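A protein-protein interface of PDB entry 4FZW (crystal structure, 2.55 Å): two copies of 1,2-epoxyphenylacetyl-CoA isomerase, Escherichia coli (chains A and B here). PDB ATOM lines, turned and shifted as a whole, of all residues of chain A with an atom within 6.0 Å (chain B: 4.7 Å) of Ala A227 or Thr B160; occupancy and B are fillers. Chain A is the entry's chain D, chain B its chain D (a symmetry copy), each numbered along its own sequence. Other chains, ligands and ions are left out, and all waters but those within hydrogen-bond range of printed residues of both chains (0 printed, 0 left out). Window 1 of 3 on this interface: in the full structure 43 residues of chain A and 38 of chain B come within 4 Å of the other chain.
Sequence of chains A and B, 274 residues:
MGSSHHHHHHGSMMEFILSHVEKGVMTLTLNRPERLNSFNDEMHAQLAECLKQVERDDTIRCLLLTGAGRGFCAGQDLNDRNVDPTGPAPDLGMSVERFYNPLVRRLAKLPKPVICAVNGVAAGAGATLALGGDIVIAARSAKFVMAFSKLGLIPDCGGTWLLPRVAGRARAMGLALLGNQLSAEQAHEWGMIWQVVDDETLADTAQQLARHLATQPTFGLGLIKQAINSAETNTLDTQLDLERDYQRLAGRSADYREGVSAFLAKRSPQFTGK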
ATOM      1  N   GLY A 222     -21.277  18.517   5.508  1.00  0.00           N
ATOM      2  CA  GLY A 222     -21.516  18.049   6.872  1.00  0.00           C
ATOM      3  C   GLY A 222     -22.158  19.083   7.793  1.00  0.00           C
ATOM      4  O   GLY A 222     -22.971  18.745   8.649  1.00  0.00           O
ATOM      5  N   LEU A 223     -21.802  20.351   7.606  1.00  0.00           N
ATOM      6  CA  LEU A 223     -22.418  21.448   8.349  1.00  0.00           C
ATOM      7  C   LEU A 223     -23.833  21.734   7.870  1.00  0.00           C
ATOM      8  O   LEU A 223     -24.719  22.082   8.668  1.00  0.00           O
ATOM      9  CB  LEU A 223     -21.597  22.729   8.197  1.00  0.00           C
ATOM     10  CG  LEU A 223     -20.148  22.690   8.655  1.00  0.00           C
ATOM     11  CD1 LEU A 223     -19.430  23.967   8.255  1.00  0.00           C
ATOM     12  CD2 LEU A 223     -20.135  22.466  10.166  1.00  0.00           C
ATOM     13  N   ILE A 224     -24.027  21.613   6.557  1.00  0.00           N
ATOM     14  CA  ILE A 224     -25.334  21.821   5.962  1.00  0.00           C
ATOM     15  C   ILE A 224     -26.305  20.825   6.580  1.00  0.00           C
ATOM     16  O   ILE A 224     -27.378  21.203   7.060  1.00  0.00           O
ATOM     17  CB  ILE A 224     -25.272  21.718   4.407  1.00  0.00           C
ATOM     18  CG1 ILE A 224     -24.639  22.981   3.822  1.00  0.00           C
ATOM     19  CG2 ILE A 224     -26.662  21.518   3.796  1.00  0.00           C
ATOM     20  CD1 ILE A 224     -24.420  22.915   2.367  1.00  0.00           C
ATOM     21  N   LYS A 225     -25.891  19.560   6.610  1.00  0.00           N
ATOM     22  CA  LYS A 225     -26.720  18.461   7.101  1.00  0.00           C
ATOM     23  C   LYS A 225     -27.058  18.632   8.586  1.00  0.00           C
ATOM     24  O   LYS A 225     -28.204  18.425   9.008  1.00  0.00           O
ATOM     25  CB  LYS A 225     -25.992  17.139   6.853  1.00  0.00           C
ATOM     26  CG  LYS A 225     -26.722  15.899   7.335  1.00  0.00           C
ATOM     27  CD  LYS A 225     -25.780  14.703   7.330  1.00  0.00           C
ATOM     28  CE  LYS A 225     -26.412  13.549   8.077  1.00  0.00           C
ATOM     29  NZ  LYS A 225     -25.736  12.245   7.804  1.00  0.00           N
ATOM     30  N   GLN A 226     -26.047  19.020   9.366  1.00  0.00           N
ATOM     31  CA  GLN A 226     -26.219  19.315  10.784  1.00  0.00           C
ATOM     32  C   GLN A 226     -27.120  20.506  11.003  1.00  0.00           C
ATOM     33  O   GLN A 226     -28.017  20.459  11.856  1.00  0.00           O
ATOM     34  CB  GLN A 226     -24.870  19.560  11.466  1.00  0.00           C
ATOM     35  CG  GLN A 226     -24.013  18.313  11.586  1.00  0.00           C
ATOM     36  CD  GLN A 226     -24.835  17.103  11.998  1.00  0.00           C
ATOM     37  OE1 GLN A 226     -25.393  17.062  13.096  1.00  0.00           O
ATOM     38  NE2 GLN A 226     -24.936  16.122  11.104  1.00  0.00           N
ATOM     39  N   ALA A 227     -26.898  21.573  10.241  1.00  0.00           N
ATOM     40  CA  ALA A 227     -27.722  22.767  10.411  1.00  0.00           C
ATOM     41  C   ALA A 227     -29.208  22.430  10.197  1.00  0.00           C
ATOM     42  O   ALA A 227     -30.063  22.770  11.018  1.00  0.00           O
ATOM     43  CB  ALA A 227     -27.263  23.875   9.463  1.00  0.00           C
ATOM     44  N   ILE A 228     -29.488  21.765   9.076  1.00  0.00           N
ATOM     45  CA  ILE A 228     -30.844  21.389   8.686  1.00  0.00           C
ATOM     46  C   ILE A 228     -31.479  20.431   9.684  1.00  0.00           C
ATOM     47  O   ILE A 228     -32.627  20.616  10.059  1.00  0.00           O
ATOM     48  CB  ILE A 228     -30.881  20.792   7.252  1.00  0.00           C
ATOM     49  CG1 ILE A 228     -30.692  21.917   6.229  1.00  0.00           C
ATOM     50  CG2 ILE A 228     -32.192  20.033   7.012  1.00  0.00           C
ATOM     51  CD1 ILE A 228     -30.312  21.453   4.893  1.00  0.00           C
ATOM     52  N   ASN A 229     -30.735  19.420  10.123  1.00  0.00           N
ATOM     53  CA  ASN A 229     -31.169  18.602  11.261  1.00  0.00           C
ATOM     54  C   ASN A 229     -31.547  19.463  12.489  1.00  0.00           C
ATOM     55  O   ASN A 229     -32.602  19.290  13.083  1.00  0.00           O
ATOM     56  CB  ASN A 229     -30.076  17.596  11.654  1.00  0.00           C
ATOM     57  CG  ASN A 229     -29.957  16.434  10.673  1.00  0.00           C
ATOM     58  OD1 ASN A 229     -30.589  16.425   9.622  1.00  0.00           O
ATOM     59  ND2 ASN A 229     -29.134  15.454  11.014  1.00  0.00           N
ATOM     60  N   SER A 230     -30.683  20.401  12.852  1.00  0.00           N
ATOM     61  CA  SER A 230     -30.877  21.180  14.072  1.00  0.00           C
ATOM     62  C   SER A 230     -32.048  22.153  13.986  1.00  0.00           C
ATOM     63  O   SER A 230     -32.628  22.556  15.018  1.00  0.00           O
ATOM     64  CB  SER A 230     -29.591  21.938  14.439  1.00  0.00           C
ATOM     65  OG  SER A 230     -28.554  21.033  14.804  1.00  0.00           O
ATOM     66  N   ALA A 231     -32.377  22.545  12.760  1.00  0.00           N
ATOM     67  CA  ALA A 231     -33.315  23.640  12.579  1.00  0.00           C
ATOM     68  C   ALA A 231     -34.709  23.159  12.940  1.00  0.00           C
ATOM     69  O   ALA A 231     -35.595  23.959  13.204  1.00  0.00           O
ATOM     70  CB  ALA A 231     -33.274  24.177  11.169  1.00  0.00           C
ATOM     71  N   GLU A 232     -34.893  21.842  12.937  1.00  0.00           N
ATOM     72  CA  GLU A 232     -36.181  21.236  13.233  1.00  0.00           C
ATOM     73  C   GLU A 232     -36.667  21.624  14.618  1.00  0.00           C
ATOM     74  O   GLU A 232     -37.877  21.732  14.848  1.00  0.00           O
ATOM     75  CB  GLU A 232     -36.087  19.716  13.107  1.00  0.00           C
ATOM     76  CG  GLU A 232     -35.726  19.255  11.703  1.00  0.00           C
ATOM     77  CD  GLU A 232     -36.843  19.510  10.673  1.00  0.00           C
ATOM     78  OE1 GLU A 232     -37.993  19.792  11.072  1.00  0.00           O
ATOM     79  OE2 GLU A 232     -36.565  19.431   9.465  1.00  0.00           O
ATOM     80  N   GLN A 239     -31.338  29.709  15.285  1.00  0.00           N
ATOM     81  CA  GLN A 239     -30.786  29.175  14.056  1.00  0.00           C
ATOM     82  C   GLN A 239     -29.906  30.164  13.293  1.00  0.00           C
ATOM     83  O   GLN A 239     -29.061  29.745  12.496  1.00  0.00           O
ATOM     84  CB  GLN A 239     -31.897  28.612  13.138  1.00  0.00           C
ATOM     85  CG  GLN A 239     -31.374  27.774  11.971  1.00  0.00           C
ATOM     86  CD  GLN A 239     -30.799  26.434  12.404  1.00  0.00           C
ATOM     87  OE1 GLN A 239     -31.075  25.953  13.486  1.00  0.00           O
ATOM     88  NE2 GLN A 239     -30.001  25.822  11.543  1.00  0.00           N
ATOM     89  N   LEU A 242     -26.560  29.862  14.779  1.00  0.00           N
ATOM     90  CA  LEU A 242     -25.882  28.628  14.387  1.00  0.00           C
ATOM     91  C   LEU A 242     -25.359  28.729  12.964  1.00  0.00           C
ATOM     92  O   LEU A 242     -24.366  28.102  12.638  1.00  0.00           O
ATOM     93  CB  LEU A 242     -26.788  27.408  14.522  1.00  0.00           C
ATOM     94  CG  LEU A 242     -26.119  26.068  14.191  1.00  0.00           C
ATOM     95  CD1 LEU A 242     -25.367  25.536  15.426  1.00  0.00           C
ATOM     96  CD2 LEU A 242     -27.115  25.038  13.702  1.00  0.00           C
ATOM     97  N   GLU A 243     -26.029  29.522  12.122  1.00  0.00           N
ATOM     98  CA  GLU A 243     -25.614  29.708  10.719  1.00  0.00           C
ATOM     99  C   GLU A 243     -24.368  30.605  10.643  1.00  0.00           C
ATOM    100  O   GLU A 243     -23.397  30.312   9.921  1.00  0.00           O
ATOM    101  CB  GLU A 243     -26.747  30.291   9.843  1.00  0.00           C
ATOM    102  CG  GLU A 243     -27.957  29.418   9.636  1.00  0.00           C
ATOM    103  CD  GLU A 243     -28.925  29.958   8.554  1.00  0.00           C
ATOM    104  OE1 GLU A 243     -29.700  29.145   7.989  1.00  0.00           O
ATOM    105  OE2 GLU A 243     -28.906  31.175   8.263  1.00  0.00           O
ATOM    106  N   TYR A 246     -21.654  28.342  11.630  1.00  0.00           N
ATOM    107  CA  TYR A 246     -21.235  27.378  10.619  1.00  0.00           C
ATOM    108  C   TYR A 246     -20.589  28.060   9.410  1.00  0.00           C
ATOM    109  O   TYR A 246     -19.665  27.533   8.801  1.00  0.00           O
ATOM    110  CB  TYR A 246     -22.401  26.482  10.205  1.00  0.00           C
ATOM    111  CG  TYR A 246     -22.716  25.382  11.208  1.00  0.00           C
ATOM    112  CD1 TYR A 246     -21.999  25.256  12.397  1.00  0.00           C
ATOM    113  CD2 TYR A 246     -23.720  24.462  10.953  1.00  0.00           C
ATOM    114  CE1 TYR A 246     -22.297  24.245  13.303  1.00  0.00           C
ATOM    115  CE2 TYR A 246     -24.018  23.455  11.840  1.00  0.00           C
ATOM    116  CZ  TYR A 246     -23.316  23.341  13.004  1.00  0.00           C
ATOM    117  OH  TYR A 246     -23.647  22.315  13.872  1.00  0.00           O
ATOM    118  N   PRO B 155     -26.207  27.524   3.470  1.00  0.00           N
ATOM    119  CA  PRO B 155     -27.290  28.471   3.183  1.00  0.00           C
ATOM    120  C   PRO B 155     -27.516  29.357   4.403  1.00  0.00           C
ATOM    121  O   PRO B 155     -27.755  28.880   5.512  1.00  0.00           O
ATOM    122  CB  PRO B 155     -28.503  27.566   2.966  1.00  0.00           C
ATOM    123  CG  PRO B 155     -27.934  26.228   2.632  1.00  0.00           C
ATOM    124  CD  PRO B 155     -26.691  26.132   3.468  1.00  0.00           C
ATOM    125  N   GLY B 158     -31.231  32.547   7.341  1.00  0.00           N
ATOM    126  CA  GLY B 158     -32.347  31.697   7.715  1.00  0.00           C
ATOM    127  C   GLY B 158     -32.580  30.569   6.732  1.00  0.00           C
ATOM    128  O   GLY B 158     -33.556  29.835   6.854  1.00  0.00           O
ATOM    129  N   GLY B 159     -31.688  30.433   5.753  1.00  0.00           N
ATOM    130  CA  GLY B 159     -31.785  29.362   4.773  1.00  0.00           C
ATOM    131  C   GLY B 159     -32.111  28.031   5.422  1.00  0.00           C
ATOM    132  O   GLY B 159     -33.125  27.396   5.081  1.00  0.00           O
ATOM    133  N   THR B 160     -31.281  27.627   6.388  1.00  0.00           N
ATOM    134  CA  THR B 160     -31.386  26.294   6.997  1.00  0.00           C
ATOM    135  C   THR B 160     -32.545  26.171   7.981  1.00  0.00           C
ATOM    136  O   THR B 160     -32.933  25.070   8.378  1.00  0.00           O
ATOM    137  CB  THR B 160     -30.072  25.893   7.663  1.00  0.00           C
ATOM    138  OG1 THR B 160     -29.768  26.822   8.712  1.00  0.00           O
ATOM    139  CG2 THR B 160     -28.942  25.896   6.627  1.00  0.00           C
ATOM    140  N   TRP B 161     -33.083  27.320   8.377  1.00  0.00           N
ATOM    141  CA  TRP B 161     -34.326  27.339   9.128  1.00  0.00           C
ATOM    142  C   TRP B 161     -35.544  27.167   8.197  1.00  0.00           C
ATOM    143  O   TRP B 161     -36.437  26.351   8.469  1.00  0.00           O
ATOM    144  CB  TRP B 161     -34.464  28.626   9.927  1.00  0.00           C
ATOM    145  CG  TRP B 161     -35.483  28.512  11.008  1.00  0.00           C
ATOM    146  CD1 TRP B 161     -35.320  27.914  12.234  1.00  0.00           C
ATOM    147  CD2 TRP B 161     -36.831  28.988  10.971  1.00  0.00           C
ATOM    148  NE1 TRP B 161     -36.484  27.991  12.959  1.00  0.00           N
ATOM    149  CE2 TRP B 161     -37.427  28.654  12.218  1.00  0.00           C
ATOM    150  CE3 TRP B 161     -37.595  29.665  10.008  1.00  0.00           C
ATOM    151  CZ2 TRP B 161     -38.755  28.977  12.525  1.00  0.00           C
ATOM    152  CZ3 TRP B 161     -38.911  29.981  10.305  1.00  0.00           C
ATOM    153  CH2 TRP B 161     -39.478  29.645  11.565  1.00  0.00           C
ATOM    154  N   LEU B 162     -35.558  27.937   7.106  1.00  0.00           N
ATOM    155  CA  LEU B 162     -36.689  28.020   6.189  1.00  0.00           C
ATOM    156  C   LEU B 162     -36.948  26.773   5.377  1.00  0.00           C
ATOM    157  O   LEU B 162     -38.096  26.378   5.240  1.00  0.00           O
ATOM    158  CB  LEU B 162     -36.490  29.155   5.184  1.00  0.00           C
ATOM    159  CG  LEU B 162     -36.745  30.574   5.668  1.00  0.00           C
ATOM    160  CD1 LEU B 162     -36.357  31.532   4.556  1.00  0.00           C
ATOM    161  CD2 LEU B 162     -38.211  30.735   6.055  1.00  0.00           C
ATOM    162  N   LEU B 163     -35.901  26.189   4.794  1.00  0.00           N
ATOM    163  CA  LEU B 163     -36.090  25.180   3.743  1.00  0.00           C
ATOM    164  C   LEU B 163     -36.901  23.988   4.211  1.00  0.00           C
ATOM    165  O   LEU B 163     -37.766  23.514   3.464  1.00  0.00           O
ATOM    166  CB  LEU B 163     -34.771  24.720   3.115  1.00  0.00           C
ATOM    167  CG  LEU B 163     -34.046  25.805   2.326  1.00  0.00           C
ATOM    168  CD1 LEU B 163     -32.671  25.330   1.887  1.00  0.00           C
ATOM    169  CD2 LEU B 163     -34.891  26.205   1.141  1.00  0.00           C
ATOM    170  N   PRO B 164     -36.643  23.509   5.452  1.00  0.00           N
ATOM    171  CA  PRO B 164     -37.351  22.324   5.956  1.00  0.00           C
ATOM    172  C   PRO B 164     -38.840  22.599   6.177  1.00  0.00           C
ATOM    173  O   PRO B 164     -39.658  21.700   6.059  1.00  0.00           O
ATOM    174  CB  PRO B 164     -36.638  22.023   7.296  1.00  0.00           C
ATOM    175  CG  PRO B 164     -35.317  22.710   7.191  1.00  0.00           C
ATOM    176  CD  PRO B 164     -35.632  23.973   6.415  1.00  0.00           C
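Printed residues of chain B that touch a printed residue of chain A: Pro B155, Gly B158, Gly B159, Thr B160, Trp B161 and Pro B164. Hydrophobic or aromatic side chains of chain B that line the printed part of chain A: Pro B155, Trp B161 and Pro B164. Hydrophobic or aromatic side chains of chain A within 4 Å of the printed part of chain B: Ile A224, Ala A227 and Ala A231. Among the printed residues, 12 pairs touch across the chains. Among the printed residues, no Asp or Glu carboxylate lies within 4 Å of a Lys or Arg side-chain nitrogen of the other chain.
Ala A227 touches just one residue of chain B: Thr B160. Thr B160 touches four residues of chain A. Of the printed residues of chain B, Glu A232 touches Pro B164 (3.4 Å). Printed residues of chain B within 4 Å of Ala A231: Thr B160 (3.0 Å) and Trp B161 (3.9 Å). Of the printed residues of chain B, Ile A224 touches Pro B155 (3.8 Å). Of the printed residues of chain A, Pro B164 touches Glu A232 (3.4 Å). Printed residues of chain B within 4 Å of Gln A239: Thr B160 and Trp B161. Tyr A246 touches none of the printed residues of chain B. Ile A228 touches none of the printed residues of chain B. The nearest printed residue of chain B that does not touch Ala A227 is Trp B161 (6.1 Å). The nearest residue of chain A that does not touch Thr B160 is Ile A228 (4.2 Å).
No position is printed for both chains.
The side-chain carboxylate of Glu A243 lies within hydrogen-bond range of the side-chain hydroxyl of Thr B160, at 2.4 Å. The side-chain carboxylate (OE2) of Glu A243 lies within hydrogen-bond range of the backbone NH (N) of Gly B158 (2.9 Å). OE1 of Glu A243 sits at hydrogen-bond distance from N of Gly B159, 3.3 Å away. OG1 of Thr B160 is in hydrogen-bond range of NE2 of Gln A239 (3.0 Å). The side-chain carboxylate (OE1) of Glu A243 sits close to the backbone carbonyl oxygen (O) of Pro B155 (3.2 Å).
The side-chain amide nitrogen (NE2) of Gln A239 is in hydrogen-bond range of the backbone carbonyl oxygen (O) of Ala A227, at 3.1 Å.
Pro B155 touches Ile A224. CG2 of Thr B160 touches CB of Ala A227 (3.9 Å). CB of Ala A231 touches O of Thr B160 (3.0 Å). Ala A231 touches Trp B161 (CB to CA, 3.9 Å). Pro B164 touches Glu A232 (CB to OE2, 3.4 Å). Trp B161 touches Gln A239. Trp B161 touches Glu A243.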
